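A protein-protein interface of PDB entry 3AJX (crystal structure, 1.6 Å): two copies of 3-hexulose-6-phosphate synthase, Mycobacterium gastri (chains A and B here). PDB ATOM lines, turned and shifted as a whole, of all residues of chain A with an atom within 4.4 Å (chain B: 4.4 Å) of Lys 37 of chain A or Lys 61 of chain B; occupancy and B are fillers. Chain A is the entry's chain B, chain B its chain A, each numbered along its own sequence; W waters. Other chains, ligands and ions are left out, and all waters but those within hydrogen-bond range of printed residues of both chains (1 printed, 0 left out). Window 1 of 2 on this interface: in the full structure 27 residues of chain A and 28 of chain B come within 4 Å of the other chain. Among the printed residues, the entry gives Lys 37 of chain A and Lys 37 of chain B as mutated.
Among the printed residues, merely in contact across the chains: Thr 33 of chain A with Glu 69 of chain B (3.9 Å), Ile 36 of chain A with Lys 37 of chain B (3.9 Å), Lys 37 of chain A with Ile 36 of chain B (3.8 Å), Lys 37 of chain A with Gly 40 of chain B (3.2 Å), Lys 37 of chain A with Lys 61 of chain B (3.9 Å), Lys 37 of chain A with Thr 62 of chain B (3.97 Å), Ala 38 of chain A with Gly 40 of chain B (3.5 Å), Glu 39 of chain A with Gly 40 of chain B (3.7 Å) and Met 63 of chain A with Leu 84 of chain B (3.97 Å).
Water W1 lies within hydrogen-bond range of the backbone carbonyl oxygen (O) of Ala 38 of chain A (3.3 Å) and the backbone NH (N) of Leu 41 of chain B (3.3 Å).
Of chain B, only Ile 36, Gly 40, Leu 41, Met 60, Lys 61, Thr 62 and Glu 69 come within 4 Å of Lys 37 of chain A. Of chain A, only Lys 37 (3.9 Å) comes within 4 Å of Lys 61 of chain B. Of the printed residues of chain A, Lys 37 of chain B touches Ile 36. Of the printed residues of chain B, Glu 39 of chain A touches Gly 40 (3.7 Å). Printed residues of chain B within 4 Å of Thr 33 of chain A: Glu 69. Printed residues of chain A within 4 Å of Glu 69 of chain B: Thr 33 and Lys 37. Of the printed residues of chain A, Leu 84 of chain B touches Met 63 (3.97 Å). Asp 59 of chain B touches none of the printed residues of chain A. The nearest printed residue of chain A that does not touch Met 60 of chain B is Ala 38 of chain A (6.1 Å).
Ile 36 of chain A touches Lys 37 of chain B, and with the chains exchanged Lys 37 of chain A touches Ile 36 of chain B.
O of Lys 37 of chain A lies within hydrogen-bond range of N of Leu 41 of chain B, at 3.1 Å. O of Ala 38 of chain A lies within hydrogen-bond range of N of Leu 41 of chain B, 3.2 Å away. The side-chain amino group (NZ) of Lys 37 of chain A lies within hydrogen-bond range of the backbone carbonyl oxygen (O) of Met 60 of chain B (2.7 Å). NZ of Lys 37 of chain A is in salt-bridge range of OE1 of Glu 69 of chain B (2.8 Å).
The side-chain amino group (NZ) of Lys 61 of chain B is in hydrogen-bond range of the side-chain hydroxyl (OG1) of Thr 33 of chain B, 2.9 Å away. The side-chain carboxylate (OD1) of Asp 59 of chain B lies within salt-bridge range of the side-chain amino group (NZ) of Lys 61 of chain B (3.2 Å). The backbone NH (N) of Lys 61 of chain B is in hydrogen-bond range of the side-chain hydroxyl (OG1) of Thr 82 of chain B, 2.9 Å away. The side-chain amino group (NZ) of Lys 61 of chain B lies within salt-bridge range of the side-chain carboxylate (OD2) of Asp 109 of chain B, 3.7 Å away. N of Thr 62 of chain B sits at hydrogen-bond distance from O of Thr 82 of chain B, 3.2 Å away. The backbone carbonyl oxygen of Thr 62 of chain B sits at hydrogen-bond distance from the backbone NH of Leu 84 of chain B (2.9 Å).
Printed residues of chain A that touch a printed residue of chain B: Thr 33, Ile 36, Lys 37, Ala 38, Glu 39 and Met 63. Among the printed residues, 13 pairs touch across the chains. Among the printed residues, Asp or Glu carboxylates within 4 Å of a Lys or Arg side-chain nitrogen of the other chain: Lys 37 of chain A with Glu 69 of chain B.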
ATOM      1  N   THR A  33      -2.114   3.055  15.250  1.00  0.00           N
ATOM      2  CA  THR A  33      -3.192   3.596  14.438  1.00  0.00           C
ATOM      3  C   THR A  33      -2.715   4.425  13.248  1.00  0.00           C
ATOM      4  O   THR A  33      -3.194   4.238  12.132  1.00  0.00           O
ATOM      5  CB  THR A  33      -4.142   4.445  15.299  1.00  0.00           C
ATOM      6  OG1 THR A  33      -4.559   3.678  16.434  1.00  0.00           O
ATOM      7  CG2 THR A  33      -5.364   4.853  14.495  1.00  0.00           C
ATOM      8  N   PRO A  34      -1.774   5.361  13.462  1.00  0.00           N
ATOM      9  CA  PRO A  34      -1.319   6.152  12.315  1.00  0.00           C
ATOM     10  C   PRO A  34      -0.575   5.316  11.274  1.00  0.00           C
ATOM     11  O   PRO A  34      -0.617   5.619  10.080  1.00  0.00           O
ATOM     12  CB  PRO A  34      -0.443   7.226  12.960  1.00  0.00           C
ATOM     13  CG  PRO A  34       0.093   6.540  14.174  1.00  0.00           C
ATOM     14  CD  PRO A  34      -1.128   5.818  14.705  1.00  0.00           C
ATOM     15  N   LEU A  35       0.098   4.261  11.730  1.00  0.00           N
ATOM     16  CA  LEU A  35       0.831   3.380  10.825  1.00  0.00           C
ATOM     17  C   LEU A  35      -0.148   2.616   9.939  1.00  0.00           C
ATOM     18  O   LEU A  35       0.078   2.467   8.740  1.00  0.00           O
ATOM     19  CB  LEU A  35       1.695   2.391  11.618  1.00  0.00           C
ATOM     20  CG  LEU A  35       2.389   1.278  10.823  1.00  0.00           C
ATOM     21  CD1 LEU A  35       3.284   1.862   9.736  1.00  0.00           C
ATOM     22  CD2 LEU A  35       3.200   0.420  11.775  1.00  0.00           C
ATOM     23  N   ILE A  36      -1.238   2.134  10.532  1.00  0.00           N
ATOM     24  CA  ILE A  36      -2.244   1.403   9.769  1.00  0.00           C
ATOM     25  C   ILE A  36      -2.922   2.330   8.759  1.00  0.00           C
ATOM     26  O   ILE A  36      -3.212   1.923   7.634  1.00  0.00           O
ATOM     27  CB  ILE A  36      -3.307   0.767  10.700  1.00  0.00           C
ATOM     28  CG1 ILE A  36      -2.668  -0.362  11.518  1.00  0.00           C
ATOM     29  CG2 ILE A  36      -4.468   0.221   9.873  1.00  0.00           C
ATOM     30  CD1 ILE A  36      -3.592  -0.980  12.562  1.00  0.00           C
ATOM     31  N   LYS A  37      -3.161   3.581   9.143  1.00  0.00           N
ATOM     32  CA  LYS A  37      -3.801   4.514   8.223  1.00  0.00           C
ATOM     33  C   LYS A  37      -2.840   4.956   7.129  1.00  0.00           C
ATOM     34  O   LYS A  37      -3.255   5.303   6.026  1.00  0.00           O
ATOM     35  CB  LYS A  37      -4.342   5.730   8.978  1.00  0.00           C
ATOM     36  CG  LYS A  37      -5.481   5.373   9.916  1.00  0.00           C
ATOM     37  CD  LYS A  37      -5.966   6.576  10.684  1.00  0.00           C
ATOM     38  CE  LYS A  37      -7.057   6.181  11.650  1.00  0.00           C
ATOM     39  NZ  LYS A  37      -7.441   7.328  12.506  1.00  0.00           N
ATOM     40  N   ALA A  38      -1.549   4.922   7.428  1.00  0.00           N
ATOM     41  CA  ALA A  38      -0.553   5.329   6.451  1.00  0.00           C
ATOM     42  C   ALA A  38      -0.296   4.252   5.401  1.00  0.00           C
ATOM     43  O   ALA A  38      -0.284   4.538   4.202  1.00  0.00           O
ATOM     44  CB  ALA A  38       0.753   5.677   7.159  1.00  0.00           C
ATOM     45  N   GLU A  39      -0.112   3.016   5.857  1.00  0.00           N
ATOM     46  CA  GLU A  39       0.198   1.895   4.973  1.00  0.00           C
ATOM     47  C   GLU A  39      -0.936   0.928   4.655  1.00  0.00           C
ATOM     48  O   GLU A  39      -0.881   0.217   3.651  1.00  0.00           O
ATOM     49  CB  GLU A  39       1.365   1.105   5.570  1.00  0.00           C
ATOM     50  CG  GLU A  39       2.639   1.918   5.707  1.00  0.00           C
ATOM     51  CD  GLU A  39       3.370   2.066   4.389  1.00  0.00           C
ATOM     52  OE1 GLU A  39       2.707   1.983   3.332  1.00  0.00           O
ATOM     53  OE2 GLU A  39       4.602   2.271   4.411  1.00  0.00           O
ATOM     54  N   MET A  63     -14.350   2.737  15.490  1.00  0.00           N
ATOM     55  CA  MET A  63     -15.407   3.580  16.042  1.00  0.00           C
ATOM     56  C   MET A  63     -16.779   3.191  15.486  1.00  0.00           C
ATOM     57  O   MET A  63     -17.814   3.579  16.033  1.00  0.00           O
ATOM     58  CB  MET A  63     -15.108   5.051  15.739  1.00  0.00           C
ATOM     59  CG  MET A  63     -16.051   6.040  16.404  1.00  0.00           C
ATOM     60  SD  MET A  63     -16.155   5.863  18.204  1.00  0.00           S
ATOM     61  CE  MET A  63     -17.836   6.490  18.483  1.00  0.00           C
ATOM     62  N   THR B  33     -13.511   5.279   6.354  1.00  0.00           N
ATOM     63  CA  THR B  33     -12.534   4.839   7.335  1.00  0.00           C
ATOM     64  C   THR B  33     -12.020   3.425   7.047  1.00  0.00           C
ATOM     65  O   THR B  33     -10.817   3.181   7.088  1.00  0.00           O
ATOM     66  CB  THR B  33     -13.126   4.913   8.751  1.00  0.00           C
ATOM     67  OG1 THR B  33     -13.680   6.220   8.960  1.00  0.00           O
ATOM     68  CG2 THR B  33     -12.048   4.662   9.790  1.00  0.00           C
ATOM     69  N   ILE B  36      -9.549   3.503   4.082  1.00  0.00           N
ATOM     70  CA  ILE B  36      -8.240   4.044   4.414  1.00  0.00           C
ATOM     71  C   ILE B  36      -7.439   3.025   5.223  1.00  0.00           C
ATOM     72  O   ILE B  36      -6.251   2.837   4.988  1.00  0.00           O
ATOM     73  CB  ILE B  36      -8.377   5.360   5.205  1.00  0.00           C
ATOM     74  CG1 ILE B  36      -8.965   6.442   4.287  1.00  0.00           C
ATOM     75  CG2 ILE B  36      -7.015   5.790   5.761  1.00  0.00           C
ATOM     76  CD1 ILE B  36      -9.283   7.742   4.984  1.00  0.00           C
ATOM     77  N   LYS B  37      -8.082   2.351   6.168  1.00  0.00           N
ATOM     78  CA  LYS B  37      -7.365   1.365   6.969  1.00  0.00           C
ATOM     79  C   LYS B  37      -6.972   0.160   6.119  1.00  0.00           C
ATOM     80  O   LYS B  37      -5.985  -0.519   6.400  1.00  0.00           O
ATOM     81  CB  LYS B  37      -8.219   0.921   8.161  1.00  0.00           C
ATOM     82  CG  LYS B  37      -8.436   2.031   9.178  1.00  0.00           C
ATOM     83  CD  LYS B  37      -9.292   1.593  10.353  1.00  0.00           C
ATOM     84  CE  LYS B  37      -9.523   2.770  11.292  1.00  0.00           C
ATOM     85  NZ  LYS B  37     -10.425   2.442  12.427  1.00  0.00           N
ATOM     86  N   GLY B  40      -4.487   2.325   3.072  1.00  0.00           N
ATOM     87  CA  GLY B  40      -3.514   3.319   3.483  1.00  0.00           C
ATOM     88  C   GLY B  40      -3.798   4.605   2.730  1.00  0.00           C
ATOM     89  O   GLY B  40      -4.738   4.666   1.934  1.00  0.00           O
ATOM     90  N   LEU B  41      -2.976   5.625   2.960  1.00  0.00           N
ATOM     91  CA  LEU B  41      -3.148   6.934   2.332  1.00  0.00           C
ATOM     92  C   LEU B  41      -3.134   6.965   0.804  1.00  0.00           C
ATOM     93  O   LEU B  41      -3.665   7.900   0.206  1.00  0.00           O
ATOM     94  CB  LEU B  41      -2.088   7.901   2.870  1.00  0.00           C
ATOM     95  CG  LEU B  41      -2.096   8.133   4.385  1.00  0.00           C
ATOM     96  CD1 LEU B  41      -0.930   9.034   4.763  1.00  0.00           C
ATOM     97  CD2 LEU B  41      -3.417   8.756   4.810  1.00  0.00           C
ATOM     98  N   ASP B  59     -11.910  10.223   5.624  1.00  0.00           N
ATOM     99  CA  ASP B  59     -12.558   9.900   6.895  1.00  0.00           C
ATOM    100  C   ASP B  59     -11.599   9.189   7.846  1.00  0.00           C
ATOM    101  O   ASP B  59     -11.756   8.000   8.148  1.00  0.00           O
ATOM    102  CB  ASP B  59     -13.788   9.019   6.646  1.00  0.00           C
ATOM    103  CG  ASP B  59     -14.824   9.137   7.749  1.00  0.00           C
ATOM    104  OD1 ASP B  59     -14.521   9.740   8.798  1.00  0.00           O
ATOM    105  OD2 ASP B  59     -15.947   8.621   7.565  1.00  0.00           O
ATOM    106  N   MET B  60     -10.609   9.934   8.326  1.00  0.00           N
ATOM    107  CA  MET B  60      -9.603   9.400   9.238  1.00  0.00           C
ATOM    108  C   MET B  60     -10.172   9.038  10.608  1.00  0.00           C
ATOM    109  O   MET B  60      -9.717   8.085  11.240  1.00  0.00           O
ATOM    110  CB  MET B  60      -8.483  10.430   9.426  1.00  0.00           C
ATOM    111  CG  MET B  60      -7.725  10.803   8.166  1.00  0.00           C
ATOM    112  SD  MET B  60      -6.647   9.477   7.576  1.00  0.00           S
ATOM    113  CE  MET B  60      -5.171   9.732   8.590  1.00  0.00           C
ATOM    114  N   LYS B  61     -11.175   9.796  11.050  1.00  0.00           N
ATOM    115  CA  LYS B  61     -11.780   9.599  12.367  1.00  0.00           C
ATOM    116  C   LYS B  61     -10.672   9.593  13.416  1.00  0.00           C
ATOM    117  O   LYS B  61     -10.632   8.744  14.307  1.00  0.00           O
ATOM    118  CB  LYS B  61     -12.583   8.293  12.431  1.00  0.00           C
ATOM    119  CG  LYS B  61     -13.967   8.390  11.798  1.00  0.00           C
ATOM    120  CD  LYS B  61     -14.805   7.158  12.108  1.00  0.00           C
ATOM    121  CE  LYS B  61     -16.200   7.260  11.507  1.00  0.00           C
ATOM    122  NZ  LYS B  61     -16.161   7.334  10.019  1.00  0.00           N
ATOM    123  N   THR B  62      -9.775  10.564  13.294  1.00  0.00           N
ATOM    124  CA  THR B  62      -8.652  10.699  14.211  1.00  0.00           C
ATOM    125  C   THR B  62      -9.075  10.805  15.674  1.00  0.00           C
ATOM    126  O   THR B  62      -9.988  11.555  16.018  1.00  0.00           O
ATOM    127  CB  THR B  62      -7.819  11.922  13.837  1.00  0.00           C
ATOM    128  OG1 THR B  62      -7.351  11.763  12.493  1.00  0.00           O
ATOM    129  CG2 THR B  62      -6.631  12.080  14.779  1.00  0.00           C
ATOM    130  N   MET B  63      -8.393  10.053  16.533  1.00  0.00           N
ATOM    131  CA  MET B  63      -8.700  10.064  17.957  1.00  0.00           C
ATOM    132  C   MET B  63      -7.533  10.612  18.774  1.00  0.00           C
ATOM    133  O   MET B  63      -7.710  11.041  19.911  1.00  0.00           O
ATOM    134  CB  MET B  63      -9.038   8.649  18.422  1.00  0.00           C
ATOM    135  CG  MET B  63      -9.480   8.541  19.872  1.00  0.00           C
ATOM    136  SD  MET B  63     -10.997   9.453  20.226  1.00  0.00           S
ATOM    137  CE  MET B  63     -10.858   9.632  22.007  1.00  0.00           C
ATOM    138  N   GLU B  69      -2.022  13.113  12.061  1.00  0.00           N
ATOM    139  CA  GLU B  69      -2.945  12.422  11.169  1.00  0.00           C
ATOM    140  C   GLU B  69      -3.556  13.359  10.135  1.00  0.00           C
ATOM    141  O   GLU B  69      -3.738  12.983   8.977  1.00  0.00           O
ATOM    142  CB  GLU B  69      -4.052  11.712  11.963  1.00  0.00           C
ATOM    143  CG  GLU B  69      -3.551  10.488  12.720  1.00  0.00           C
ATOM    144  CD  GLU B  69      -4.641   9.468  13.003  1.00  0.00           C
ATOM    145  OE1 GLU B  69      -5.754   9.598  12.447  1.00  0.00           O
ATOM    146  OE2 GLU B  69      -4.374   8.522  13.774  1.00  0.00           O
ATOM    147  N   THR B  82     -11.452  14.114   8.828  1.00  0.00           N
ATOM    148  CA  THR B  82     -12.297  14.026  10.009  1.00  0.00           C
ATOM    149  C   THR B  82     -11.514  13.690  11.260  1.00  0.00           C
ATOM    150  O   THR B  82     -10.547  12.926  11.223  1.00  0.00           O
ATOM    151  CB  THR B  82     -13.413  12.960   9.878  1.00  0.00           C
ATOM    152  OG1 THR B  82     -12.843  11.675   9.606  1.00  0.00           O
ATOM    153  CG2 THR B  82     -14.375  13.334   8.784  1.00  0.00           C
ATOM    154  N   LEU B  84     -12.554  12.808  15.420  1.00  0.00           N
ATOM    155  CA  LEU B  84     -13.707  12.464  16.251  1.00  0.00           C
ATOM    156  C   LEU B  84     -14.016  13.533  17.291  1.00  0.00           C
ATOM    157  O   LEU B  84     -13.114  14.099  17.903  1.00  0.00           O
ATOM    158  CB  LEU B  84     -13.470  11.136  16.974  1.00  0.00           C
ATOM    159  CG  LEU B  84     -13.412   9.888  16.097  1.00  0.00           C
ATOM    160  CD1 LEU B  84     -13.117   8.660  16.958  1.00  0.00           C
ATOM    161  CD2 LEU B  84     -14.740   9.727  15.366  1.00  0.00           C
ATOM    162  N   ASP B 109     -16.356  14.663  13.285  1.00  0.00           N
ATOM    163  CA  ASP B 109     -17.378  13.625  13.199  1.00  0.00           C
ATOM    164  C   ASP B 109     -17.943  13.400  14.597  1.00  0.00           C
ATOM    165  O   ASP B 109     -17.239  12.923  15.489  1.00  0.00           O
ATOM    166  CB  ASP B 109     -16.751  12.331  12.667  1.00  0.00           C
ATOM    167  CG  ASP B 109     -17.782  11.282  12.327  1.00  0.00           C
ATOM    168  OD1 ASP B 109     -18.882  11.323  12.910  1.00  0.00           O
ATOM    169  OD2 ASP B 109     -17.490  10.409  11.484  1.00  0.00           O
ATOM    170  N   HIS B 134     -23.516  12.441  12.539  1.00  0.00           N
ATOM    171  CA  HIS B 134     -23.355  11.090  12.033  1.00  0.00           C
ATOM    172  C   HIS B 134     -23.865   9.940  12.897  1.00  0.00           C
ATOM    173  O   HIS B 134     -23.630   9.896  14.106  1.00  0.00           O
ATOM    174  CB  HIS B 134     -21.856  10.902  11.768  1.00  0.00           C
ATOM    175  CG  HIS B 134     -21.506   9.655  11.022  1.00  0.00           C
ATOM    176  ND1 HIS B 134     -20.200   9.243  10.853  1.00  0.00           N
ATOM    177  CD2 HIS B 134     -22.275   8.744  10.384  1.00  0.00           C
ATOM    178  CE1 HIS B 134     -20.185   8.129  10.144  1.00  0.00           C
ATOM    179  NE2 HIS B 134     -21.429   7.805   9.845  1.00  0.00           N
HETATM  180  O   HOH W   1      -1.171   3.485   1.251  1.00  0.00           O
